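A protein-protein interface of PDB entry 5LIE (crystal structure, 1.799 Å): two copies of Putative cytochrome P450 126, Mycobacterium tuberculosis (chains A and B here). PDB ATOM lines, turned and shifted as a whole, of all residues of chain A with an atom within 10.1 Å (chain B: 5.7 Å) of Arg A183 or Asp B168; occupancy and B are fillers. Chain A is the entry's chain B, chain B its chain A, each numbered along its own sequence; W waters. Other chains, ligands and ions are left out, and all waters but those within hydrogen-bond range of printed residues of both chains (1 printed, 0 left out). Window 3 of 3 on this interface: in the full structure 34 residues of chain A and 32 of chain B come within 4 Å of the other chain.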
ATOM      1  N   ASP A  16       1.384 -31.513  10.109  1.00  0.00           N
ATOM      2  CA  ASP A  16       1.746 -30.912  11.404  1.00  0.00           C
ATOM      3  C   ASP A  16       1.657 -31.966  12.506  1.00  0.00           C
ATOM      4  O   ASP A  16       2.443 -31.930  13.460  1.00  0.00           O
ATOM      5  CB  ASP A  16       0.813 -29.755  11.774  1.00  0.00           C
ATOM      6  CG  ASP A  16       1.182 -28.428  11.085  1.00  0.00           C
ATOM      7  OD1 ASP A  16       2.280 -28.333  10.480  1.00  0.00           O
ATOM      8  OD2 ASP A  16       0.360 -27.464  11.169  1.00  0.00           O
ATOM      9  N   PHE A 180      14.321 -33.951   0.463  1.00  0.00           N
ATOM     10  CA  PHE A 180      14.542 -32.576   0.013  1.00  0.00           C
ATOM     11  C   PHE A 180      13.933 -31.599   1.003  1.00  0.00           C
ATOM     12  O   PHE A 180      13.022 -31.954   1.712  1.00  0.00           O
ATOM     13  CB  PHE A 180      13.928 -32.345  -1.369  1.00  0.00           C
ATOM     14  CG  PHE A 180      12.436 -32.580  -1.432  1.00  0.00           C
ATOM     15  CD1 PHE A 180      11.551 -31.518  -1.371  1.00  0.00           C
ATOM     16  CD2 PHE A 180      11.918 -33.876  -1.580  1.00  0.00           C
ATOM     17  CE1 PHE A 180      10.179 -31.723  -1.463  1.00  0.00           C
ATOM     18  CE2 PHE A 180      10.553 -34.086  -1.672  1.00  0.00           C
ATOM     19  CZ  PHE A 180       9.676 -33.000  -1.612  1.00  0.00           C
ATOM     20  N   ASP A 181      14.421 -30.362   1.020  1.00  0.00           N
ATOM     21  CA  ASP A 181      13.860 -29.360   1.892  1.00  0.00           C
ATOM     22  C   ASP A 181      12.694 -28.690   1.201  1.00  0.00           C
ATOM     23  O   ASP A 181      12.795 -28.314   0.034  1.00  0.00           O
ATOM     24  CB  ASP A 181      14.910 -28.299   2.198  1.00  0.00           C
ATOM     25  CG  ASP A 181      14.404 -27.244   3.203  1.00  0.00           C
ATOM     26  OD1 ASP A 181      14.707 -27.398   4.413  1.00  0.00           O
ATOM     27  OD2 ASP A 181      13.695 -26.277   2.793  1.00  0.00           O
ATOM     28  N   PHE A 182      11.622 -28.471   1.942  1.00  0.00           N
ATOM     29  CA  PHE A 182      10.501 -27.684   1.436  1.00  0.00           C
ATOM     30  C   PHE A 182       9.926 -26.855   2.579  1.00  0.00           C
ATOM     31  O   PHE A 182       9.429 -27.404   3.560  1.00  0.00           O
ATOM     32  CB  PHE A 182       9.393 -28.564   0.846  1.00  0.00           C
ATOM     33  CG  PHE A 182       8.243 -27.762   0.230  1.00  0.00           C
ATOM     34  CD1 PHE A 182       8.463 -26.975  -0.887  1.00  0.00           C
ATOM     35  CD2 PHE A 182       6.964 -27.797   0.786  1.00  0.00           C
ATOM     36  CE1 PHE A 182       7.400 -26.221  -1.455  1.00  0.00           C
ATOM     37  CE2 PHE A 182       5.900 -27.068   0.222  1.00  0.00           C
ATOM     38  CZ  PHE A 182       6.131 -26.276  -0.889  1.00  0.00           C
ATOM     39  N   ARG A 183       9.969 -25.531   2.434  1.00  0.00           N
ATOM     40  CA  ARG A 183       9.503 -24.612   3.483  1.00  0.00           C
ATOM     41  C   ARG A 183      10.194 -24.911   4.830  1.00  0.00           C
ATOM     42  O   ARG A 183       9.592 -24.735   5.887  1.00  0.00           O
ATOM     43  CB  ARG A 183       7.982 -24.647   3.622  1.00  0.00           C
ATOM     44  CG  ARG A 183       7.217 -24.196   2.357  1.00  0.00           C
ATOM     45  CD  ARG A 183       5.711 -23.999   2.660  1.00  0.00           C
ATOM     46  NE  ARG A 183       4.914 -23.664   1.472  1.00  0.00           N
ATOM     47  CZ  ARG A 183       4.911 -22.475   0.879  1.00  0.00           C
ATOM     48  NH1 ARG A 183       5.683 -21.498   1.344  1.00  0.00           N
ATOM     49  NH2 ARG A 183       4.145 -22.260  -0.188  1.00  0.00           N
ATOM     50  N   GLY A 184      11.458 -25.354   4.770  1.00  0.00           N
ATOM     51  CA  GLY A 184      12.279 -25.493   5.961  1.00  0.00           C
ATOM     52  C   GLY A 184      12.214 -26.863   6.639  1.00  0.00           C
ATOM     53  O   GLY A 184      12.930 -27.085   7.633  1.00  0.00           O
ATOM     54  N   SER A 185      11.359 -27.753   6.132  1.00  0.00           N
ATOM     55  CA  SER A 185      11.263 -29.134   6.655  1.00  0.00           C
ATOM     56  C   SER A 185      11.762 -30.153   5.632  1.00  0.00           C
ATOM     57  O   SER A 185      11.667 -29.933   4.431  1.00  0.00           O
ATOM     58  CB  SER A 185       9.822 -29.490   7.004  1.00  0.00           C
ATOM     59  OG  SER A 185       9.360 -28.740   8.121  1.00  0.00           O
ATOM     60  N   ARG A 186      12.293 -31.282   6.096  1.00  0.00           N
ATOM     61  CA  ARG A 186      12.662 -32.317   5.150  1.00  0.00           C
ATOM     62  C   ARG A 186      11.456 -33.139   4.720  1.00  0.00           C
ATOM     63  O   ARG A 186      10.656 -33.577   5.553  1.00  0.00           O
ATOM     64  CB  ARG A 186      13.734 -33.234   5.735  1.00  0.00           C
ATOM     65  CG  ARG A 186      14.192 -34.335   4.783  1.00  0.00           C
ATOM     66  CD  ARG A 186      15.319 -35.160   5.470  1.00  0.00           C
ATOM     67  NE  ARG A 186      15.943 -36.121   4.568  1.00  0.00           N
ATOM     68  CZ  ARG A 186      15.478 -37.340   4.383  1.00  0.00           C
ATOM     69  NH1 ARG A 186      14.385 -37.729   5.027  1.00  0.00           N
ATOM     70  NH2 ARG A 186      16.108 -38.165   3.555  1.00  0.00           N
ATOM     71  N   ARG A 187      11.341 -33.385   3.414  1.00  0.00           N
ATOM     72  CA  ARG A 187      10.278 -34.236   2.875  1.00  0.00           C
ATOM     73  C   ARG A 187      10.872 -35.398   2.104  1.00  0.00           C
ATOM     74  O   ARG A 187      12.053 -35.385   1.756  1.00  0.00           O
ATOM     75  CB  ARG A 187       9.403 -33.419   1.895  1.00  0.00           C
ATOM     76  CG  ARG A 187       8.849 -32.106   2.482  1.00  0.00           C
ATOM     77  CD  ARG A 187       7.745 -32.369   3.474  1.00  0.00           C
ATOM     78  NE  ARG A 187       6.562 -32.918   2.817  1.00  0.00           N
ATOM     79  CZ  ARG A 187       5.557 -32.181   2.342  1.00  0.00           C
ATOM     80  NH1 ARG A 187       5.579 -30.864   2.486  1.00  0.00           N
ATOM     81  NH2 ARG A 187       4.527 -32.773   1.750  1.00  0.00           N
ATOM     82  N   GLU A 394      15.205 -33.369  15.264  1.00  0.00           N
ATOM     83  CA  GLU A 394      14.303 -32.797  14.280  1.00  0.00           C
ATOM     84  C   GLU A 394      13.809 -33.923  13.387  1.00  0.00           C
ATOM     85  O   GLU A 394      14.610 -34.756  12.980  1.00  0.00           O
ATOM     86  CB  GLU A 394      15.003 -31.717  13.452  1.00  0.00           C
ATOM     87  CG  GLU A 394      14.061 -31.153  12.386  1.00  0.00           C
ATOM     88  CD  GLU A 394      14.641 -29.998  11.594  1.00  0.00           C
ATOM     89  OE1 GLU A 394      13.934 -29.533  10.673  1.00  0.00           O
ATOM     90  OE2 GLU A 394      15.776 -29.559  11.880  1.00  0.00           O
ATOM     91  N   ARG A 397       9.294 -34.422   7.913  1.00  0.00           N
ATOM     92  CA  ARG A 397       7.857 -34.142   7.886  1.00  0.00           C
ATOM     93  C   ARG A 397       7.126 -35.109   6.916  1.00  0.00           C
ATOM     94  O   ARG A 397       7.038 -34.890   5.694  1.00  0.00           O
ATOM     95  CB  ARG A 397       7.642 -32.665   7.507  1.00  0.00           C
ATOM     96  CG  ARG A 397       6.215 -32.207   7.487  1.00  0.00           C
ATOM     97  CD  ARG A 397       6.186 -30.727   7.114  1.00  0.00           C
ATOM     98  NE  ARG A 397       4.823 -30.228   7.060  1.00  0.00           N
ATOM     99  CZ  ARG A 397       4.170 -29.700   8.094  1.00  0.00           C
ATOM    100  NH1 ARG A 397       4.766 -29.551   9.284  1.00  0.00           N
ATOM    101  NH2 ARG A 397       2.928 -29.278   7.902  1.00  0.00           N
ATOM    102  N   ARG A 405      15.612 -36.196  10.978  1.00  0.00           N
ATOM    103  CA  ARG A 405      16.434 -35.405  10.071  1.00  0.00           C
ATOM    104  C   ARG A 405      17.803 -35.098  10.665  1.00  0.00           C
ATOM    105  O   ARG A 405      18.807 -35.107   9.964  1.00  0.00           O
ATOM    106  CB  ARG A 405      15.740 -34.088   9.819  1.00  0.00           C
ATOM    107  CG  ARG A 405      16.445 -33.238   8.791  1.00  0.00           C
ATOM    108  CD  ARG A 405      15.709 -31.879   8.661  1.00  0.00           C
ATOM    109  NE  ARG A 405      16.146 -31.175   7.462  1.00  0.00           N
ATOM    110  CZ  ARG A 405      15.680 -29.988   7.072  1.00  0.00           C
ATOM    111  NH1 ARG A 405      14.775 -29.346   7.803  1.00  0.00           N
ATOM    112  NH2 ARG A 405      16.139 -29.449   5.945  1.00  0.00           N
ATOM    113  N   VAL B 164      -1.246 -18.607  -9.503  1.00  0.00           N
ATOM    114  CA  VAL B 164      -0.120 -18.642  -8.531  1.00  0.00           C
ATOM    115  C   VAL B 164       0.118 -17.247  -7.924  1.00  0.00           C
ATOM    116  O   VAL B 164       0.478 -16.306  -8.642  1.00  0.00           O
ATOM    117  CB  VAL B 164       1.199 -18.996  -9.211  1.00  0.00           C
ATOM    118  CG1 VAL B 164       2.346 -19.026  -8.200  1.00  0.00           C
ATOM    119  CG2 VAL B 164       1.134 -20.370  -9.927  1.00  0.00           C
ATOM    120  N   PRO B 165      -0.021 -17.117  -6.597  1.00  0.00           N
ATOM    121  CA  PRO B 165       0.207 -15.822  -5.896  1.00  0.00           C
ATOM    122  C   PRO B 165       1.639 -15.291  -6.026  1.00  0.00           C
ATOM    123  O   PRO B 165       2.555 -16.075  -6.109  1.00  0.00           O
ATOM    124  CB  PRO B 165      -0.058 -16.173  -4.422  1.00  0.00           C
ATOM    125  CG  PRO B 165      -0.828 -17.477  -4.426  1.00  0.00           C
ATOM    126  CD  PRO B 165      -0.405 -18.203  -5.683  1.00  0.00           C
ATOM    127  N   GLU B 166       1.863 -13.977  -5.996  1.00  0.00           N
ATOM    128  CA  GLU B 166       3.235 -13.438  -6.089  1.00  0.00           C
ATOM    129  C   GLU B 166       4.217 -14.086  -5.113  1.00  0.00           C
ATOM    130  O   GLU B 166       5.373 -14.362  -5.465  1.00  0.00           O
ATOM    131  CB  GLU B 166       3.208 -11.925  -5.856  1.00  0.00           C
ATOM    132  CG  GLU B 166       4.588 -11.300  -5.682  1.00  0.00           C
ATOM    133  CD  GLU B 166       4.553  -9.771  -5.639  1.00  0.00           C
ATOM    134  OE1 GLU B 166       3.637  -9.165  -6.256  1.00  0.00           O
ATOM    135  OE2 GLU B 166       5.452  -9.179  -4.989  1.00  0.00           O
ATOM    136  N   THR B 167       3.764 -14.343  -3.889  1.00  0.00           N
ATOM    137  CA  THR B 167       4.635 -14.869  -2.834  1.00  0.00           C
ATOM    138  C   THR B 167       5.252 -16.220  -3.183  1.00  0.00           C
ATOM    139  O   THR B 167       6.298 -16.620  -2.624  1.00  0.00           O
ATOM    140  CB  THR B 167       3.850 -15.095  -1.514  1.00  0.00           C
ATOM    141  OG1 THR B 167       2.962 -13.997  -1.271  1.00  0.00           O
ATOM    142  CG2 THR B 167       4.812 -15.233  -0.357  1.00  0.00           C
ATOM    143  N   ASP B 168       4.580 -16.935  -4.081  1.00  0.00           N
ATOM    144  CA  ASP B 168       4.913 -18.336  -4.352  1.00  0.00           C
ATOM    145  C   ASP B 168       5.504 -18.541  -5.735  1.00  0.00           C
ATOM    146  O   ASP B 168       5.822 -19.682  -6.136  1.00  0.00           O
ATOM    147  CB  ASP B 168       3.644 -19.189  -4.196  1.00  0.00           C
ATOM    148  CG  ASP B 168       3.231 -19.366  -2.742  1.00  0.00           C
ATOM    149  OD1 ASP B 168       4.131 -19.560  -1.889  1.00  0.00           O
ATOM    150  OD2 ASP B 168       2.022 -19.357  -2.457  1.00  0.00           O
ATOM    151  N   ARG B 169       5.673 -17.454  -6.475  1.00  0.00           N
ATOM    152  CA  ARG B 169       6.203 -17.572  -7.827  1.00  0.00           C
ATOM    153  C   ARG B 169       7.654 -18.051  -7.867  1.00  0.00           C
ATOM    154  O   ARG B 169       8.105 -18.641  -8.855  1.00  0.00           O
ATOM    155  CB  ARG B 169       5.982 -16.253  -8.578  1.00  0.00           C
ATOM    156  CG  ARG B 169       4.519 -15.996  -8.680  1.00  0.00           C
ATOM    157  CD  ARG B 169       4.148 -14.812  -9.501  1.00  0.00           C
ATOM    158  NE  ARG B 169       2.702 -14.778  -9.668  1.00  0.00           N
ATOM    159  CZ  ARG B 169       2.000 -13.689  -9.954  1.00  0.00           C
ATOM    160  NH1 ARG B 169       2.633 -12.521 -10.062  1.00  0.00           N
ATOM    161  NH2 ARG B 169       0.675 -13.768 -10.113  1.00  0.00           N
ATOM    162  N   HIS B 170       8.399 -17.861  -6.782  1.00  0.00           N
ATOM    163  CA  HIS B 170       9.796 -18.263  -6.807  1.00  0.00           C
ATOM    164  C   HIS B 170       9.963 -19.782  -7.005  1.00  0.00           C
ATOM    165  O   HIS B 170      10.969 -20.237  -7.542  1.00  0.00           O
ATOM    166  CB  HIS B 170      10.491 -17.860  -5.513  1.00  0.00           C
ATOM    167  CG  HIS B 170      10.091 -18.683  -4.330  1.00  0.00           C
ATOM    168  ND1 HIS B 170       8.983 -18.399  -3.560  1.00  0.00           N
ATOM    169  CD2 HIS B 170      10.655 -19.786  -3.783  1.00  0.00           C
ATOM    170  CE1 HIS B 170       8.883 -19.289  -2.586  1.00  0.00           C
ATOM    171  NE2 HIS B 170       9.882 -20.146  -2.703  1.00  0.00           N
ATOM    172  N   TRP B 171       9.008 -20.572  -6.528  1.00  0.00           N
ATOM    173  CA  TRP B 171       9.110 -22.041  -6.697  1.00  0.00           C
ATOM    174  C   TRP B 171       9.202 -22.352  -8.185  1.00  0.00           C
ATOM    175  O   TRP B 171       9.938 -23.261  -8.623  1.00  0.00           O
ATOM    176  CB  TRP B 171       7.885 -22.798  -6.124  1.00  0.00           C
ATOM    177  CG  TRP B 171       7.569 -22.552  -4.691  1.00  0.00           C
ATOM    178  CD1 TRP B 171       6.444 -21.977  -4.200  1.00  0.00           C
ATOM    179  CD2 TRP B 171       8.389 -22.870  -3.545  1.00  0.00           C
ATOM    180  NE1 TRP B 171       6.500 -21.902  -2.826  1.00  0.00           N
ATOM    181  CE2 TRP B 171       7.682 -22.452  -2.401  1.00  0.00           C
ATOM    182  CE3 TRP B 171       9.646 -23.467  -3.386  1.00  0.00           C
ATOM    183  CZ2 TRP B 171       8.188 -22.596  -1.111  1.00  0.00           C
ATOM    184  CZ3 TRP B 171      10.158 -23.613  -2.099  1.00  0.00           C
ATOM    185  CH2 TRP B 171       9.429 -23.174  -0.981  1.00  0.00           C
ATOM    186  N   LEU B 172       8.458 -21.572  -8.957  1.00  0.00           N
ATOM    187  CA  LEU B 172       8.395 -21.812 -10.386  1.00  0.00           C
ATOM    188  C   LEU B 172       9.662 -21.331 -11.046  1.00  0.00           C
ATOM    189  O   LEU B 172      10.246 -22.052 -11.835  1.00  0.00           O
ATOM    190  CB  LEU B 172       7.171 -21.103 -10.993  1.00  0.00           C
ATOM    191  CG  LEU B 172       5.890 -21.944 -10.879  1.00  0.00           C
ATOM    192  CD1 LEU B 172       5.400 -22.080  -9.392  1.00  0.00           C
ATOM    193  CD2 LEU B 172       4.783 -21.327 -11.772  1.00  0.00           C
ATOM    194  N   TYR B 205       4.913 -28.041  -4.221  1.00  0.00           N
ATOM    195  CA  TYR B 205       4.206 -26.746  -4.191  1.00  0.00           C
ATOM    196  C   TYR B 205       2.947 -26.862  -5.084  1.00  0.00           C
ATOM    197  O   TYR B 205       1.865 -26.438  -4.702  1.00  0.00           O
ATOM    198  CB  TYR B 205       5.095 -25.596  -4.695  1.00  0.00           C
ATOM    199  CG  TYR B 205       4.206 -24.404  -4.923  1.00  0.00           C
ATOM    200  CD1 TYR B 205       3.616 -23.769  -3.847  1.00  0.00           C
ATOM    201  CD2 TYR B 205       3.841 -24.014  -6.216  1.00  0.00           C
ATOM    202  CE1 TYR B 205       2.706 -22.723  -4.022  1.00  0.00           C
ATOM    203  CE2 TYR B 205       2.954 -22.937  -6.413  1.00  0.00           C
ATOM    204  CZ  TYR B 205       2.397 -22.309  -5.313  1.00  0.00           C
ATOM    205  OH  TYR B 205       1.511 -21.282  -5.486  1.00  0.00           O
ATOM    206  N   GLU B 208       0.190 -28.509  -3.381  1.00  0.00           N
ATOM    207  CA  GLU B 208      -0.366 -27.601  -2.364  1.00  0.00           C
ATOM    208  C   GLU B 208      -1.322 -26.567  -2.994  1.00  0.00           C
ATOM    209  O   GLU B 208      -2.413 -26.304  -2.506  1.00  0.00           O
ATOM    210  CB  GLU B 208       0.814 -26.886  -1.695  1.00  0.00           C
ATOM    211  CG  GLU B 208       0.480 -26.014  -0.514  1.00  0.00           C
ATOM    212  CD  GLU B 208       1.650 -25.092  -0.178  1.00  0.00           C
ATOM    213  OE1 GLU B 208       2.608 -25.540   0.483  1.00  0.00           O
ATOM    214  OE2 GLU B 208       1.617 -23.922  -0.626  1.00  0.00           O
HETATM  215  O   HOH W   1       6.654 -19.266  -0.539  1.00  0.00           O
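The side-chain carboxylate (OD1) of Asp B168 lies within salt-bridge range of the guanidinium group (NH2) of Arg A183. The side-chain carboxylate (OE2) of Glu B208 lies within salt-bridge range of the guanidinium group (NH2) of Arg A183, at 3.1 Å.
The indole nitrogen (NE1) of Trp B171 lies within hydrogen-bond range of the side-chain carboxylate (OD1) of Asp B168 (3.5 Å).
Trp B171 touches Phe A182 (CH2 to CE1, 3.7 Å). Phe A182 touches Tyr B205. CE2 of Phe A182 touches OE1 of Glu B208 (3.6 Å). Arg A183 touches Trp B171. Tyr B205 touches Arg A183 (CD1 to NH2, 3.99 Å).
Of the printed residues of chain B, Arg A183 touches Asp B168, Trp B171, Tyr B205 and Glu B208. Asp B168 touches one residue of chain A. No residue of chain A comes within 4 Å of His B170. Of the printed residues of chain B, Phe A182 touches Trp B171, Tyr B205 and Glu B208. Of the printed residues of chain A, Tyr B205 touches Phe A182 (3.9 Å) and Arg A183 (3.99 Å). Of the printed residues of chain A, Glu B208 touches Phe A182 and Arg A183. The nearest printed residue of chain B that does not touch Arg A183 is His B170 (5.5 Å). The nearest residue of chain A that does not touch Asp B168 is Phe A182 (7.1 Å).
Of the 11 printed residues of chain B, 4 touch a printed residue of chain A. Hydrophobic or aromatic side chains of chain B within 4 Å of the printed part of chain A: Trp B171 and Tyr B205. Printed residues of chain A that touch a printed residue of chain B: Phe A182 and Arg A183.
No position is printed for both chains. Of the 7 pairs that touch across the chains among the printed residues, none has its exchanged pair printed and touching as well.
Water W1 lies within hydrogen-bond range of OD1 of Asp B168 (2.9 Å), NH1 of Arg A183 (3.1 Å), O of Thr B167 (3.4 Å) and NE1 of Trp B171 (3.5 Å).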
